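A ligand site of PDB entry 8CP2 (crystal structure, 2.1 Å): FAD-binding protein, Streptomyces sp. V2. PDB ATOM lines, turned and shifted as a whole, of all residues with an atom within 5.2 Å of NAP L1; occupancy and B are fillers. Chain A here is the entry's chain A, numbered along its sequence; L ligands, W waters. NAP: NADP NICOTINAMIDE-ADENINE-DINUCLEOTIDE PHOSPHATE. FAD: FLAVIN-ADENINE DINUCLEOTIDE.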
ATOM      1  N   LEU A  60      24.393  19.724 -17.580  1.00  0.00           N
ATOM      2  CA  LEU A  60      25.416  20.347 -18.453  1.00  0.00           C
ATOM      3  C   LEU A  60      25.244  21.867 -18.406  1.00  0.00           C
ATOM      4  O   LEU A  60      24.156  22.342 -18.152  1.00  0.00           O
ATOM      5  CB  LEU A  60      25.209  19.860 -19.904  1.00  0.00           C
ATOM      6  CG  LEU A  60      25.422  18.382 -20.177  1.00  0.00           C
ATOM      7  CD1 LEU A  60      25.129  18.112 -21.668  1.00  0.00           C
ATOM      8  CD2 LEU A  60      26.835  17.945 -19.786  1.00  0.00           C
ATOM      9  N   MET A  61      26.288  22.588 -18.782  1.00  0.00           N
ATOM     10  CA  MET A  61      26.208  23.993 -19.201  1.00  0.00           C
ATOM     11  C   MET A  61      25.664  24.073 -20.634  1.00  0.00           C
ATOM     12  O   MET A  61      25.556  23.065 -21.330  1.00  0.00           O
ATOM     13  CB  MET A  61      27.580  24.654 -19.150  1.00  0.00           C
ATOM     14  CG  MET A  61      28.207  24.643 -17.787  1.00  0.00           C
ATOM     15  SD  MET A  61      29.742  25.685 -17.774  1.00  0.00           S
ATOM     16  CE  MET A  61      29.019  27.321 -17.937  1.00  0.00           C
ATOM     17  N   ASN A  62      25.337  25.295 -21.025  1.00  0.00           N
ATOM     18  CA  ASN A  62      24.849  25.719 -22.356  1.00  0.00           C
ATOM     19  C   ASN A  62      25.912  26.547 -23.099  1.00  0.00           C
ATOM     20  O   ASN A  62      25.615  27.043 -24.178  1.00  0.00           O
ATOM     21  CB  ASN A  62      23.611  26.600 -22.165  1.00  0.00           C
ATOM     22  CG  ASN A  62      22.678  26.296 -23.270  1.00  0.00           C
ATOM     23  OD1 ASN A  62      22.609  25.130 -23.642  1.00  0.00           O
ATOM     24  ND2 ASN A  62      22.077  27.317 -23.841  1.00  0.00           N
ATOM     25  N   ARG A 104      27.880  21.035 -15.101  1.00  0.00           N
ATOM     26  CA  ARG A 104      27.757  22.159 -14.159  1.00  0.00           C
ATOM     27  C   ARG A 104      28.681  21.944 -12.984  1.00  0.00           C
ATOM     28  O   ARG A 104      29.321  22.951 -12.523  1.00  0.00           O
ATOM     29  CB  ARG A 104      26.315  22.314 -13.743  1.00  0.00           C
ATOM     30  CG  ARG A 104      25.413  22.841 -14.852  1.00  0.00           C
ATOM     31  CD  ARG A 104      24.245  23.554 -14.088  1.00  0.00           C
ATOM     32  NE  ARG A 104      23.311  23.344 -15.076  1.00  0.00           N
ATOM     33  CZ  ARG A 104      22.117  22.799 -15.026  1.00  0.00           C
ATOM     34  NH1 ARG A 104      21.408  22.610 -13.935  1.00  0.00           N
ATOM     35  NH2 ARG A 104      21.598  22.579 -16.199  1.00  0.00           N
ATOM     36  N   PRO A 197      16.602  22.587 -11.662  1.00  0.00           N
ATOM     37  CA  PRO A 197      16.404  21.132 -11.691  1.00  0.00           C
ATOM     38  C   PRO A 197      17.401  20.399 -10.793  1.00  0.00           C
ATOM     39  O   PRO A 197      17.000  19.414 -10.199  1.00  0.00           O
ATOM     40  CB  PRO A 197      16.594  20.750 -13.178  1.00  0.00           C
ATOM     41  CG  PRO A 197      16.208  22.009 -13.907  1.00  0.00           C
ATOM     42  CD  PRO A 197      16.752  23.119 -13.031  1.00  0.00           C
ATOM     43  N   ARG A 214       5.906  20.650 -17.579  1.00  0.00           N
ATOM     44  CA  ARG A 214       5.283  21.882 -18.156  1.00  0.00           C
ATOM     45  C   ARG A 214       6.420  22.886 -18.471  1.00  0.00           C
ATOM     46  O   ARG A 214       6.957  23.470 -17.504  1.00  0.00           O
ATOM     47  CB  ARG A 214       4.283  22.524 -17.193  1.00  0.00           C
ATOM     48  CG  ARG A 214       3.732  23.847 -17.729  1.00  0.00           C
ATOM     49  CD  ARG A 214       2.311  24.200 -17.402  1.00  0.00           C
ATOM     50  NE  ARG A 214       2.040  24.209 -15.974  1.00  0.00           N
ATOM     51  CZ  ARG A 214       0.829  24.322 -15.445  1.00  0.00           C
ATOM     52  NH1 ARG A 214      -0.205  24.508 -16.249  1.00  0.00           N
ATOM     53  NH2 ARG A 214       0.670  24.269 -14.124  1.00  0.00           N
ATOM     54  N   GLY A 215       6.804  23.005 -19.733  1.00  0.00           N
ATOM     55  CA  GLY A 215       8.033  23.706 -20.174  1.00  0.00           C
ATOM     56  C   GLY A 215       8.856  22.842 -21.124  1.00  0.00           C
ATOM     57  O   GLY A 215       8.876  21.609 -20.918  1.00  0.00           O
ATOM     58  N   LEU A 216       9.486  23.474 -22.135  1.00  0.00           N
ATOM     59  CA  LEU A 216      10.254  22.824 -23.229  1.00  0.00           C
ATOM     60  C   LEU A 216      11.567  23.572 -23.509  1.00  0.00           C
ATOM     61  O   LEU A 216      12.158  23.409 -24.616  1.00  0.00           O
ATOM     62  CB  LEU A 216       9.366  22.765 -24.478  1.00  0.00           C
ATOM     63  CG  LEU A 216       8.259  21.712 -24.415  1.00  0.00           C
ATOM     64  CD1 LEU A 216       7.353  21.785 -25.627  1.00  0.00           C
ATOM     65  CD2 LEU A 216       8.826  20.323 -24.290  1.00  0.00           C
ATOM     66  N   GLY A 217      12.067  24.277 -22.493  1.00  0.00           N
ATOM     67  CA  GLY A 217      13.297  25.092 -22.557  1.00  0.00           C
ATOM     68  C   GLY A 217      14.428  24.424 -21.843  1.00  0.00           C
ATOM     69  O   GLY A 217      14.419  23.176 -21.755  1.00  0.00           O
ATOM     70  N   LEU A 218      15.379  25.177 -21.309  1.00  0.00           N
ATOM     71  CA  LEU A 218      16.586  24.523 -20.763  1.00  0.00           C
ATOM     72  C   LEU A 218      16.249  23.684 -19.507  1.00  0.00           C
ATOM     73  O   LEU A 218      16.898  22.669 -19.322  1.00  0.00           O
ATOM     74  CB  LEU A 218      17.667  25.597 -20.543  1.00  0.00           C
ATOM     75  CG  LEU A 218      18.224  26.207 -21.838  1.00  0.00           C
ATOM     76  CD1 LEU A 218      19.375  27.146 -21.519  1.00  0.00           C
ATOM     77  CD2 LEU A 218      18.717  25.108 -22.792  1.00  0.00           C
ATOM     78  N   ASN A 219      15.334  24.094 -18.643  1.00  0.00           N
ATOM     79  CA  ASN A 219      14.951  23.261 -17.464  1.00  0.00           C
ATOM     80  C   ASN A 219      14.364  21.915 -17.926  1.00  0.00           C
ATOM     81  O   ASN A 219      14.698  20.902 -17.313  1.00  0.00           O
ATOM     82  CB  ASN A 219      13.896  23.921 -16.557  1.00  0.00           C
ATOM     83  CG  ASN A 219      14.503  24.741 -15.444  1.00  0.00           C
ATOM     84  OD1 ASN A 219      15.576  25.339 -15.627  1.00  0.00           O
ATOM     85  ND2 ASN A 219      13.848  24.774 -14.286  1.00  0.00           N
ATOM     86  N   PHE A 220      13.544  21.936 -18.963  1.00  0.00           N
ATOM     87  CA  PHE A 220      13.010  20.723 -19.615  1.00  0.00           C
ATOM     88  C   PHE A 220      14.147  19.766 -19.935  1.00  0.00           C
ATOM     89  O   PHE A 220      14.033  18.608 -19.540  1.00  0.00           O
ATOM     90  CB  PHE A 220      12.218  21.056 -20.867  1.00  0.00           C
ATOM     91  CG  PHE A 220      12.006  19.860 -21.747  1.00  0.00           C
ATOM     92  CD1 PHE A 220      11.127  18.852 -21.354  1.00  0.00           C
ATOM     93  CD2 PHE A 220      12.690  19.725 -22.944  1.00  0.00           C
ATOM     94  CE1 PHE A 220      10.931  17.729 -22.148  1.00  0.00           C
ATOM     95  CE2 PHE A 220      12.494  18.602 -23.739  1.00  0.00           C
ATOM     96  CZ  PHE A 220      11.614  17.614 -23.346  1.00  0.00           C
ATOM     97  N   ASP A 222      17.143  19.502 -18.720  1.00  0.00           N
ATOM     98  CA  ASP A 222      17.716  18.936 -17.472  1.00  0.00           C
ATOM     99  C   ASP A 222      16.819  17.772 -16.950  1.00  0.00           C
ATOM    100  O   ASP A 222      17.349  16.740 -16.624  1.00  0.00           O
ATOM    101  CB  ASP A 222      17.829  19.969 -16.366  1.00  0.00           C
ATOM    102  CG  ASP A 222      18.944  21.012 -16.459  1.00  0.00           C
ATOM    103  OD1 ASP A 222      19.854  20.871 -17.343  1.00  0.00           O
ATOM    104  OD2 ASP A 222      18.906  21.944 -15.597  1.00  0.00           O
ATOM    105  N   SER A 257       4.251  23.060 -23.809  1.00  0.00           N
ATOM    106  CA  SER A 257       4.315  24.504 -23.467  1.00  0.00           C
ATOM    107  C   SER A 257       3.304  25.261 -24.285  1.00  0.00           C
ATOM    108  O   SER A 257       2.563  24.642 -25.063  1.00  0.00           O
ATOM    109  CB  SER A 257       5.726  25.077 -23.678  1.00  0.00           C
ATOM    110  OG  SER A 257       6.050  25.140 -25.063  1.00  0.00           O
ATOM    111  N   ARG A 258       3.302  26.587 -24.144  1.00  0.00           N
ATOM    112  CA  ARG A 258       2.348  27.458 -24.871  1.00  0.00           C
ATOM    113  C   ARG A 258       2.755  27.389 -26.358  1.00  0.00           C
ATOM    114  O   ARG A 258       1.886  27.096 -27.178  1.00  0.00           O
ATOM    115  CB  ARG A 258       2.274  28.824 -24.153  1.00  0.00           C
ATOM    116  CG  ARG A 258       1.764  28.760 -22.712  1.00  0.00           C
ATOM    117  CD  ARG A 258       2.063  29.845 -21.644  1.00  0.00           C
ATOM    118  NE  ARG A 258       3.446  30.280 -21.495  1.00  0.00           N
ATOM    119  CZ  ARG A 258       3.816  31.246 -20.669  1.00  0.00           C
ATOM    120  NH1 ARG A 258       2.933  31.833 -19.884  1.00  0.00           N
ATOM    121  NH2 ARG A 258       5.069  31.634 -20.649  1.00  0.00           N
ATOM    122  N   ARG A 259       4.032  27.605 -26.665  1.00  0.00           N
ATOM    123  CA  ARG A 259       4.474  27.579 -28.087  1.00  0.00           C
ATOM    124  C   ARG A 259       4.439  26.119 -28.570  1.00  0.00           C
ATOM    125  O   ARG A 259       4.114  25.872 -29.719  1.00  0.00           O
ATOM    126  CB  ARG A 259       5.827  28.272 -28.257  1.00  0.00           C
ATOM    127  CG  ARG A 259       6.349  28.256 -29.686  1.00  0.00           C
ATOM    128  CD  ARG A 259       7.821  28.633 -29.794  1.00  0.00           C
ATOM    129  NE  ARG A 259       8.092  29.865 -29.050  1.00  0.00           N
ATOM    130  CZ  ARG A 259       7.898  31.085 -29.532  1.00  0.00           C
ATOM    131  NH1 ARG A 259       7.510  31.274 -30.772  1.00  0.00           N
ATOM    132  NH2 ARG A 259       8.132  32.137 -28.768  1.00  0.00           N
ATOM    133  N   GLY A 260       4.763  25.185 -27.698  1.00  0.00           N
ATOM    134  CA  GLY A 260       4.617  23.743 -27.953  1.00  0.00           C
ATOM    135  C   GLY A 260       5.861  23.099 -28.515  1.00  0.00           C
ATOM    136  O   GLY A 260       5.728  21.931 -28.921  1.00  0.00           O
ATOM    137  N   TYR A 263      13.181  24.067 -27.509  1.00  0.00           N
ATOM    138  CA  TYR A 263      14.016  25.224 -27.935  1.00  0.00           C
ATOM    139  C   TYR A 263      14.972  24.746 -29.041  1.00  0.00           C
ATOM    140  O   TYR A 263      15.279  23.546 -29.122  1.00  0.00           O
ATOM    141  CB  TYR A 263      14.705  25.819 -26.710  1.00  0.00           C
ATOM    142  CG  TYR A 263      13.827  26.776 -25.939  1.00  0.00           C
ATOM    143  CD1 TYR A 263      12.432  26.696 -25.950  1.00  0.00           C
ATOM    144  CD2 TYR A 263      14.421  27.792 -25.194  1.00  0.00           C
ATOM    145  CE1 TYR A 263      11.655  27.641 -25.278  1.00  0.00           C
ATOM    146  CE2 TYR A 263      13.668  28.709 -24.483  1.00  0.00           C
ATOM    147  CZ  TYR A 263      12.289  28.648 -24.546  1.00  0.00           C
ATOM    148  OH  TYR A 263      11.617  29.566 -23.821  1.00  0.00           O
ATOM    149  N   PRO A 439      11.025  36.163 -24.896  1.00  0.00           N
ATOM    150  CA  PRO A 439      10.693  34.751 -25.076  1.00  0.00           C
ATOM    151  C   PRO A 439      10.995  34.164 -26.455  1.00  0.00           C
ATOM    152  O   PRO A 439      11.448  33.069 -26.461  1.00  0.00           O
ATOM    153  CB  PRO A 439       9.174  34.591 -24.781  1.00  0.00           C
ATOM    154  CG  PRO A 439       8.751  35.945 -24.275  1.00  0.00           C
ATOM    155  CD  PRO A 439       9.826  36.968 -24.605  1.00  0.00           C
ATOM    156  N   ALA A 442      14.905  33.693 -26.564  1.00  0.00           N
ATOM    157  CA  ALA A 442      15.317  32.538 -25.751  1.00  0.00           C
ATOM    158  C   ALA A 442      15.070  31.253 -26.576  1.00  0.00           C
ATOM    159  O   ALA A 442      16.012  30.431 -26.694  1.00  0.00           O
ATOM    160  CB  ALA A 442      14.598  32.528 -24.405  1.00  0.00           C
ATOM    161  N   ILE A 446      18.778  30.746 -27.068  1.00  0.00           N
ATOM    162  CA  ILE A 446      19.208  30.261 -25.720  1.00  0.00           C
ATOM    163  C   ILE A 446      18.636  28.839 -25.538  1.00  0.00           C
ATOM    164  O   ILE A 446      18.128  28.451 -24.466  1.00  0.00           O
ATOM    165  CB  ILE A 446      18.838  31.257 -24.623  1.00  0.00           C
ATOM    166  CG1 ILE A 446      19.047  32.715 -25.057  1.00  0.00           C
ATOM    167  CG2 ILE A 446      19.639  30.934 -23.382  1.00  0.00           C
ATOM    168  CD1 ILE A 446      18.664  33.720 -23.999  1.00  0.00           C
ATOM    169  N   ALA A 501       8.665  23.156 -15.255  1.00  0.00           N
ATOM    170  CA  ALA A 501      10.052  23.018 -15.728  1.00  0.00           C
ATOM    171  C   ALA A 501      10.558  24.388 -16.214  1.00  0.00           C
ATOM    172  O   ALA A 501      10.654  24.594 -17.435  1.00  0.00           O
ATOM    173  CB  ALA A 501      10.143  21.948 -16.810  1.00  0.00           C
ATOM    174  N   ARG A 502      10.839  25.277 -15.268  1.00  0.00           N
ATOM    175  CA  ARG A 502      11.350  26.658 -15.463  1.00  0.00           C
ATOM    176  C   ARG A 502      11.899  27.165 -14.123  1.00  0.00           C
ATOM    177  O   ARG A 502      11.484  26.629 -13.053  1.00  0.00           O
ATOM    178  CB  ARG A 502      10.278  27.648 -15.913  1.00  0.00           C
ATOM    179  CG  ARG A 502       9.079  27.765 -15.003  1.00  0.00           C
ATOM    180  CD  ARG A 502       7.983  28.647 -15.628  1.00  0.00           C
ATOM    181  NE  ARG A 502       6.888  28.818 -14.669  1.00  0.00           N
ATOM    182  CZ  ARG A 502       5.890  27.950 -14.472  1.00  0.00           C
ATOM    183  NH1 ARG A 502       5.778  26.850 -15.224  1.00  0.00           N
ATOM    184  NH2 ARG A 502       5.027  28.155 -13.493  1.00  0.00           N
ATOM    185  N   LEU A 503      12.837  28.117 -14.188  1.00  0.00           N
ATOM    186  CA  LEU A 503      13.393  28.789 -12.985  1.00  0.00           C
ATOM    187  C   LEU A 503      12.392  29.851 -12.589  1.00  0.00           C
ATOM    188  O   LEU A 503      11.751  30.421 -13.451  1.00  0.00           O
ATOM    189  CB  LEU A 503      14.703  29.516 -13.313  1.00  0.00           C
ATOM    190  CG  LEU A 503      15.951  28.721 -13.609  1.00  0.00           C
ATOM    191  CD1 LEU A 503      17.089  29.711 -13.792  1.00  0.00           C
ATOM    192  CD2 LEU A 503      16.294  27.746 -12.516  1.00  0.00           C
ATOM    193  N   ALA A 573      21.206  36.626 -16.701  1.00  0.00           N
ATOM    194  CA  ALA A 573      21.526  35.190 -16.412  1.00  0.00           C
ATOM    195  C   ALA A 573      22.505  34.663 -17.488  1.00  0.00           C
ATOM    196  O   ALA A 573      22.072  33.952 -18.429  1.00  0.00           O
ATOM    197  CB  ALA A 573      20.235  34.374 -16.353  1.00  0.00           C
HETATM  198  PA  NAP L   1      13.526  28.823 -20.800  1.00  0.00           P
HETATM  199  O1A NAP L   1      14.723  28.043 -21.222  1.00  0.00           O
HETATM  200  O2A NAP L   1      13.192  30.093 -21.503  1.00  0.00           O
HETATM  201  O5B NAP L   1      12.231  27.839 -20.935  1.00  0.00           O
HETATM  202  C5B NAP L   1      11.003  28.159 -20.221  1.00  0.00           C
HETATM  203  C4B NAP L   1       9.910  27.216 -20.686  1.00  0.00           C
HETATM  204  O4B NAP L   1       8.735  27.331 -19.849  1.00  0.00           O
HETATM  205  C3B NAP L   1       9.416  27.467 -22.110  1.00  0.00           C
HETATM  206  O3B NAP L   1       9.046  26.249 -22.716  1.00  0.00           O
HETATM  207  C2B NAP L   1       8.154  28.316 -21.966  1.00  0.00           C
HETATM  208  O2B NAP L   1       7.570  27.890 -23.237  1.00  0.00           O
HETATM  209  C1B NAP L   1       7.640  27.817 -20.629  1.00  0.00           C
HETATM  210  N9A NAP L   1       7.062  28.803 -19.744  1.00  0.00           N
HETATM  211  C8A NAP L   1       7.710  29.929 -19.299  1.00  0.00           C
HETATM  212  N7A NAP L   1       7.024  30.613 -18.414  1.00  0.00           N
HETATM  213  C5A NAP L   1       5.907  29.835 -18.200  1.00  0.00           C
HETATM  214  C6A NAP L   1       4.813  30.011 -17.342  1.00  0.00           C
HETATM  215  N6A NAP L   1       4.750  31.061 -16.533  1.00  0.00           N
HETATM  216  N1A NAP L   1       3.852  29.048 -17.315  1.00  0.00           N
HETATM  217  C2A NAP L   1       3.981  28.018 -18.180  1.00  0.00           C
HETATM  218  N3A NAP L   1       4.966  27.750 -19.026  1.00  0.00           N
HETATM  219  C4A NAP L   1       5.900  28.714 -19.010  1.00  0.00           C
HETATM  220  O3  NAP L   1      13.566  29.062 -19.226  1.00  0.00           O
HETATM  221  PN  NAP L   1      14.144  28.101 -18.093  1.00  0.00           P
HETATM  222  O1N NAP L   1      14.061  26.662 -18.543  1.00  0.00           O
HETATM  223  O2N NAP L   1      13.502  28.639 -16.834  1.00  0.00           O
HETATM  224  O5D NAP L   1      15.659  28.514 -18.045  1.00  0.00           O
HETATM  225  C5D NAP L   1      15.938  29.913 -17.650  1.00  0.00           C
HETATM  226  C4D NAP L   1      17.433  30.140 -17.744  1.00  0.00           C
HETATM  227  O4D NAP L   1      18.096  29.315 -16.774  1.00  0.00           O
HETATM  228  C3D NAP L   1      18.099  29.761 -19.061  1.00  0.00           C
HETATM  229  O3D NAP L   1      17.876  30.753 -20.034  1.00  0.00           O
HETATM  230  C2D NAP L   1      19.543  29.667 -18.606  1.00  0.00           C
HETATM  231  O2D NAP L   1      20.107  30.963 -18.421  1.00  0.00           O
HETATM  232  C1D NAP L   1      19.361  28.913 -17.297  1.00  0.00           C
HETATM  233  N1N NAP L   1      19.386  27.407 -17.432  1.00  0.00           N
HETATM  234  C2N NAP L   1      20.389  26.815 -18.106  1.00  0.00           C
HETATM  235  C3N NAP L   1      20.537  25.458 -18.067  1.00  0.00           C
HETATM  236  C7N NAP L   1      21.729  24.878 -18.758  1.00  0.00           C
HETATM  237  O7N NAP L   1      22.841  25.390 -18.600  1.00  0.00           O
HETATM  238  N7N NAP L   1      21.514  23.750 -19.430  1.00  0.00           N
HETATM  239  C4N NAP L   1      19.586  24.648 -17.424  1.00  0.00           C
HETATM  240  C5N NAP L   1      18.467  25.241 -16.931  1.00  0.00           C
HETATM  241  C6N NAP L   1      18.442  26.616 -16.821  1.00  0.00           C
HETATM  242  P2B NAP L   1       6.542  28.884 -23.871  1.00  0.00           P
HETATM  243  O1X NAP L   1       7.745  29.721 -24.145  1.00  0.00           O
HETATM  244  O2X NAP L   1       5.738  28.727 -25.093  1.00  0.00           O
HETATM  245  O3X NAP L   1       5.687  29.226 -22.667  1.00  0.00           O
HETATM  246  PA  FAD L   2      24.426  32.931  -8.736  1.00  0.00           P
HETATM  247  O1A FAD L   2      25.359  31.997  -9.452  1.00  0.00           O
HETATM  248  O2A FAD L   2      22.947  32.697  -8.573  1.00  0.00           O
HETATM  249  O5B FAD L   2      25.095  33.112  -7.323  1.00  0.00           O
HETATM  250  C5B FAD L   2      24.380  33.861  -6.307  1.00  0.00           C
HETATM  251  C4B FAD L   2      24.840  33.386  -4.962  1.00  0.00           C
HETATM  252  O4B FAD L   2      24.374  34.308  -3.954  1.00  0.00           O
HETATM  253  C3B FAD L   2      24.340  31.994  -4.526  1.00  0.00           C
HETATM  254  O3B FAD L   2      25.438  31.205  -4.096  1.00  0.00           O
HETATM  255  C2B FAD L   2      23.447  32.247  -3.306  1.00  0.00           C
HETATM  256  O2B FAD L   2      23.600  31.235  -2.326  1.00  0.00           O
HETATM  257  C1B FAD L   2      24.018  33.575  -2.791  1.00  0.00           C
HETATM  258  N9A FAD L   2      23.073  34.352  -1.998  1.00  0.00           N
HETATM  259  C8A FAD L   2      21.848  34.870  -2.407  1.00  0.00           C
HETATM  260  N7A FAD L   2      21.220  35.508  -1.445  1.00  0.00           N
HETATM  261  C5A FAD L   2      22.105  35.429  -0.371  1.00  0.00           C
HETATM  262  C6A FAD L   2      22.009  35.937   0.933  1.00  0.00           C
HETATM  263  N6A FAD L   2      20.933  36.598   1.350  1.00  0.00           N
HETATM  264  N1A FAD L   2      23.064  35.751   1.755  1.00  0.00           N
HETATM  265  C2A FAD L   2      24.126  35.058   1.291  1.00  0.00           C
HETATM  266  N3A FAD L   2      24.301  34.496   0.082  1.00  0.00           N
HETATM  267  C4A FAD L   2      23.248  34.732  -0.702  1.00  0.00           C
HETATM  268  N1  FAD L   2      25.182  31.053 -17.616  1.00  0.00           N
HETATM  269  C2  FAD L   2      26.048  30.749 -18.571  1.00  0.00           C
HETATM  270  O2  FAD L   2      26.772  31.612 -19.046  1.00  0.00           O
HETATM  271  N3  FAD L   2      26.127  29.480 -19.102  1.00  0.00           N
HETATM  272  C4  FAD L   2      25.366  28.446 -18.627  1.00  0.00           C
HETATM  273  O4  FAD L   2      25.517  27.339 -19.109  1.00  0.00           O
HETATM  274  C4X FAD L   2      24.468  28.723 -17.568  1.00  0.00           C
HETATM  275  N5  FAD L   2      23.729  27.761 -17.057  1.00  0.00           N
HETATM  276  C5X FAD L   2      22.890  28.088 -16.015  1.00  0.00           C
HETATM  277  C6  FAD L   2      22.116  27.067 -15.449  1.00  0.00           C
HETATM  278  C7  FAD L   2      21.290  27.285 -14.384  1.00  0.00           C
HETATM  279  C7M FAD L   2      20.498  26.135 -13.802  1.00  0.00           C
HETATM  280  C8  FAD L   2      21.223  28.576 -13.825  1.00  0.00           C
HETATM  281  C8M FAD L   2      20.303  28.846 -12.683  1.00  0.00           C
HETATM  282  C9  FAD L   2      21.926  29.605 -14.405  1.00  0.00           C
HETATM  283  C9A FAD L   2      22.800  29.397 -15.485  1.00  0.00           C
HETATM  284  N10 FAD L   2      23.595  30.398 -16.052  1.00  0.00           N
HETATM  285  C10 FAD L   2      24.454  30.091 -17.086  1.00  0.00           C
HETATM  286  C1' FAD L   2      23.451  31.821 -15.672  1.00  0.00           C
HETATM  287  C2' FAD L   2      24.001  32.268 -14.329  1.00  0.00           C
HETATM  288  O2' FAD L   2      23.201  33.460 -14.026  1.00  0.00           O
HETATM  289  C3' FAD L   2      25.457  32.707 -14.388  1.00  0.00           C
HETATM  290  O3' FAD L   2      26.275  31.733 -15.042  1.00  0.00           O
HETATM  291  C4' FAD L   2      25.995  32.986 -12.977  1.00  0.00           C
HETATM  292  O4' FAD L   2      25.714  31.862 -12.158  1.00  0.00           O
HETATM  293  C5' FAD L   2      25.403  34.233 -12.342  1.00  0.00           C
HETATM  294  O5' FAD L   2      26.279  34.477 -11.200  1.00  0.00           O
HETATM  295  P   FAD L   2      25.767  35.278  -9.912  1.00  0.00           P
HETATM  296  O1P FAD L   2      25.105  36.564 -10.347  1.00  0.00           O
HETATM  297  O2P FAD L   2      26.866  35.210  -8.907  1.00  0.00           O
HETATM  298  O3P FAD L   2      24.540  34.401  -9.344  1.00  0.00           O
HETATM  299  O   HOH W   1      19.923  33.141 -20.086  1.00  0.00           O
HETATM  300  O   HOH W   2       9.856  31.138 -25.591  1.00  0.00           O
HETATM  301  O   HOH W   3       8.186  26.474 -25.504  1.00  0.00           O
HETATM  302  O   HOH W   4       4.554  31.234 -25.611  1.00  0.00           O
HETATM  303  O   HOH W   5      12.249  24.774 -19.675  1.00  0.00           O
HETATM  304  O   HOH W   6      15.865  33.030 -18.596  1.00  0.00           O
HETATM  305  O   HOH W   7       9.888  32.135 -20.801  1.00  0.00           O
HETATM  306  O   HOH W   8      16.677  29.569 -22.378  1.00  0.00           O
HETATM  307  O   HOH W   9      19.415  21.967 -20.029  1.00  0.00           O
HETATM  308  O   HOH W  10      12.511  31.004 -16.379  1.00  0.00           O
HETATM  309  O   HOH W  11       8.202  31.791 -22.986  1.00  0.00           O
HETATM  310  O   HOH W  12      15.187  31.933 -20.947  1.00  0.00           O
HETATM  311  O   HOH W  13       8.784  29.141 -26.409  1.00  0.00           O
HETATM  312  O   HOH W  14      22.632  30.768 -20.042  1.00  0.00           O
HETATM  313  O   HOH W  15       7.397  26.121 -17.421  1.00  0.00           O
HETATM  314  O   HOH W  16      23.010  22.576 -21.951  1.00  0.00           O
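Water W13 lies within hydrogen-bond range of an oxygen (O1X) of NAP L1 (2.6 Å) and the guanidinium group of Arg 259 (2.8 Å). Water W10 lies within hydrogen-bond range of an oxygen (O2N) of NAP L1 (2.6 Å) and the backbone carbonyl oxygen (O) of Leu 503 (3.1 Å). Water W8 bridges an oxygen (O1A) of NAP L1 (2.7 Å) and the backbone carbonyl oxygen (O) of Ile 446 (2.8 Å). Water W3 bridges OG of Ser 257 and O2B of NAP L1. Water W1 bridges O2D of NAP L1 (2.7 Å) and O of Ala 573 (2.8 Å). Water W2 lies within hydrogen-bond range of the backbone carbonyl oxygen (O) of Pro 439, an oxygen (O1X) of NAP L1 and the side-chain hydroxyl (OH) of Tyr 263.
N of Leu 503 sits close to ND2 of Asn 219 (3.5 Å). N of Tyr 263 is in hydrogen-bond range of O of Leu 216, at 3.1 Å. ND2 of Asn 219 sits close to N of Arg 502 (3.2 Å). The guanidinium group (NH2) of Arg 104 sits at hydrogen-bond distance from the backbone carbonyl oxygen (O) of Leu 60. The side-chain carboxylate (OD1) of Asp 222 lies within salt-bridge range of the guanidinium group (NH2) of Arg 104. The backbone NH (N) of Gly 260 is in hydrogen-bond range of the side-chain hydroxyl (OG) of Ser 257 (2.9 Å).
The guanidinium group (NH2) of Arg 104 lies close to a nitrogen (N7N) of NAP L1, 3.4 Å away. CA of Met 61 touches O7N of NAP L1, 3.7 Å away. Gly 215 touches NAP L1 (CA to O4B, 3.7 Å). CA of Gly 217 touches O5B of NAP L1, 3.4 Å away. Asp 222 touches NAP L1. Ser 257 touches NAP L1. CG2 of Ile 446 touches O3D of NAP L1, at 3.8 Å. Arg 502 touches NAP L1. Ala 573 touches NAP L1. Hydrophobic or aromatic side chains within 4 Å of NAP L1: Leu 216, Leu 218, Tyr 263, Ile 446, Leu 503 and Ala 573.
The backbone NH (N) of Arg 259 lies within hydrogen-bond range of an oxygen (O2X) of NAP L1 (2.6 Å). The backbone NH (N) of Arg 258 is in hydrogen-bond range of an oxygen (O2X) of NAP L1 (3.4 Å). An oxygen (O3X) of NAP L1 lies within salt-bridge range of the guanidinium group of Arg 258 (2.7 Å). N of Leu 503 sits at hydrogen-bond distance from O2N of NAP L1 (2.8 Å). The side-chain hydroxyl (OH) of Tyr 263 lies within hydrogen-bond range of an oxygen (O2A) of NAP L1, at 2.9 Å. The backbone NH (N) of Asn 219 lies within hydrogen-bond range of an oxygen (O1N) of NAP L1 (2.9 Å). An oxygen (O3B) of NAP L1 sits at hydrogen-bond distance from the backbone NH (N) of Leu 216 (2.9 Å). O1A of NAP L1 lies within hydrogen-bond range of N of Leu 218 (2.9 Å). The backbone carbonyl oxygen (O) of Leu 60 lies within hydrogen-bond range of a nitrogen (N7N) of NAP L1, at 3.3 Å. An oxygen (O7N) of NAP L1 is in hydrogen-bond range of the backbone NH (N) of Asn 62 (3.5 Å). An oxygen (O4) of FAD L2 is in hydrogen-bond range of the backbone NH (N) of Asn 62 (2.8 Å).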
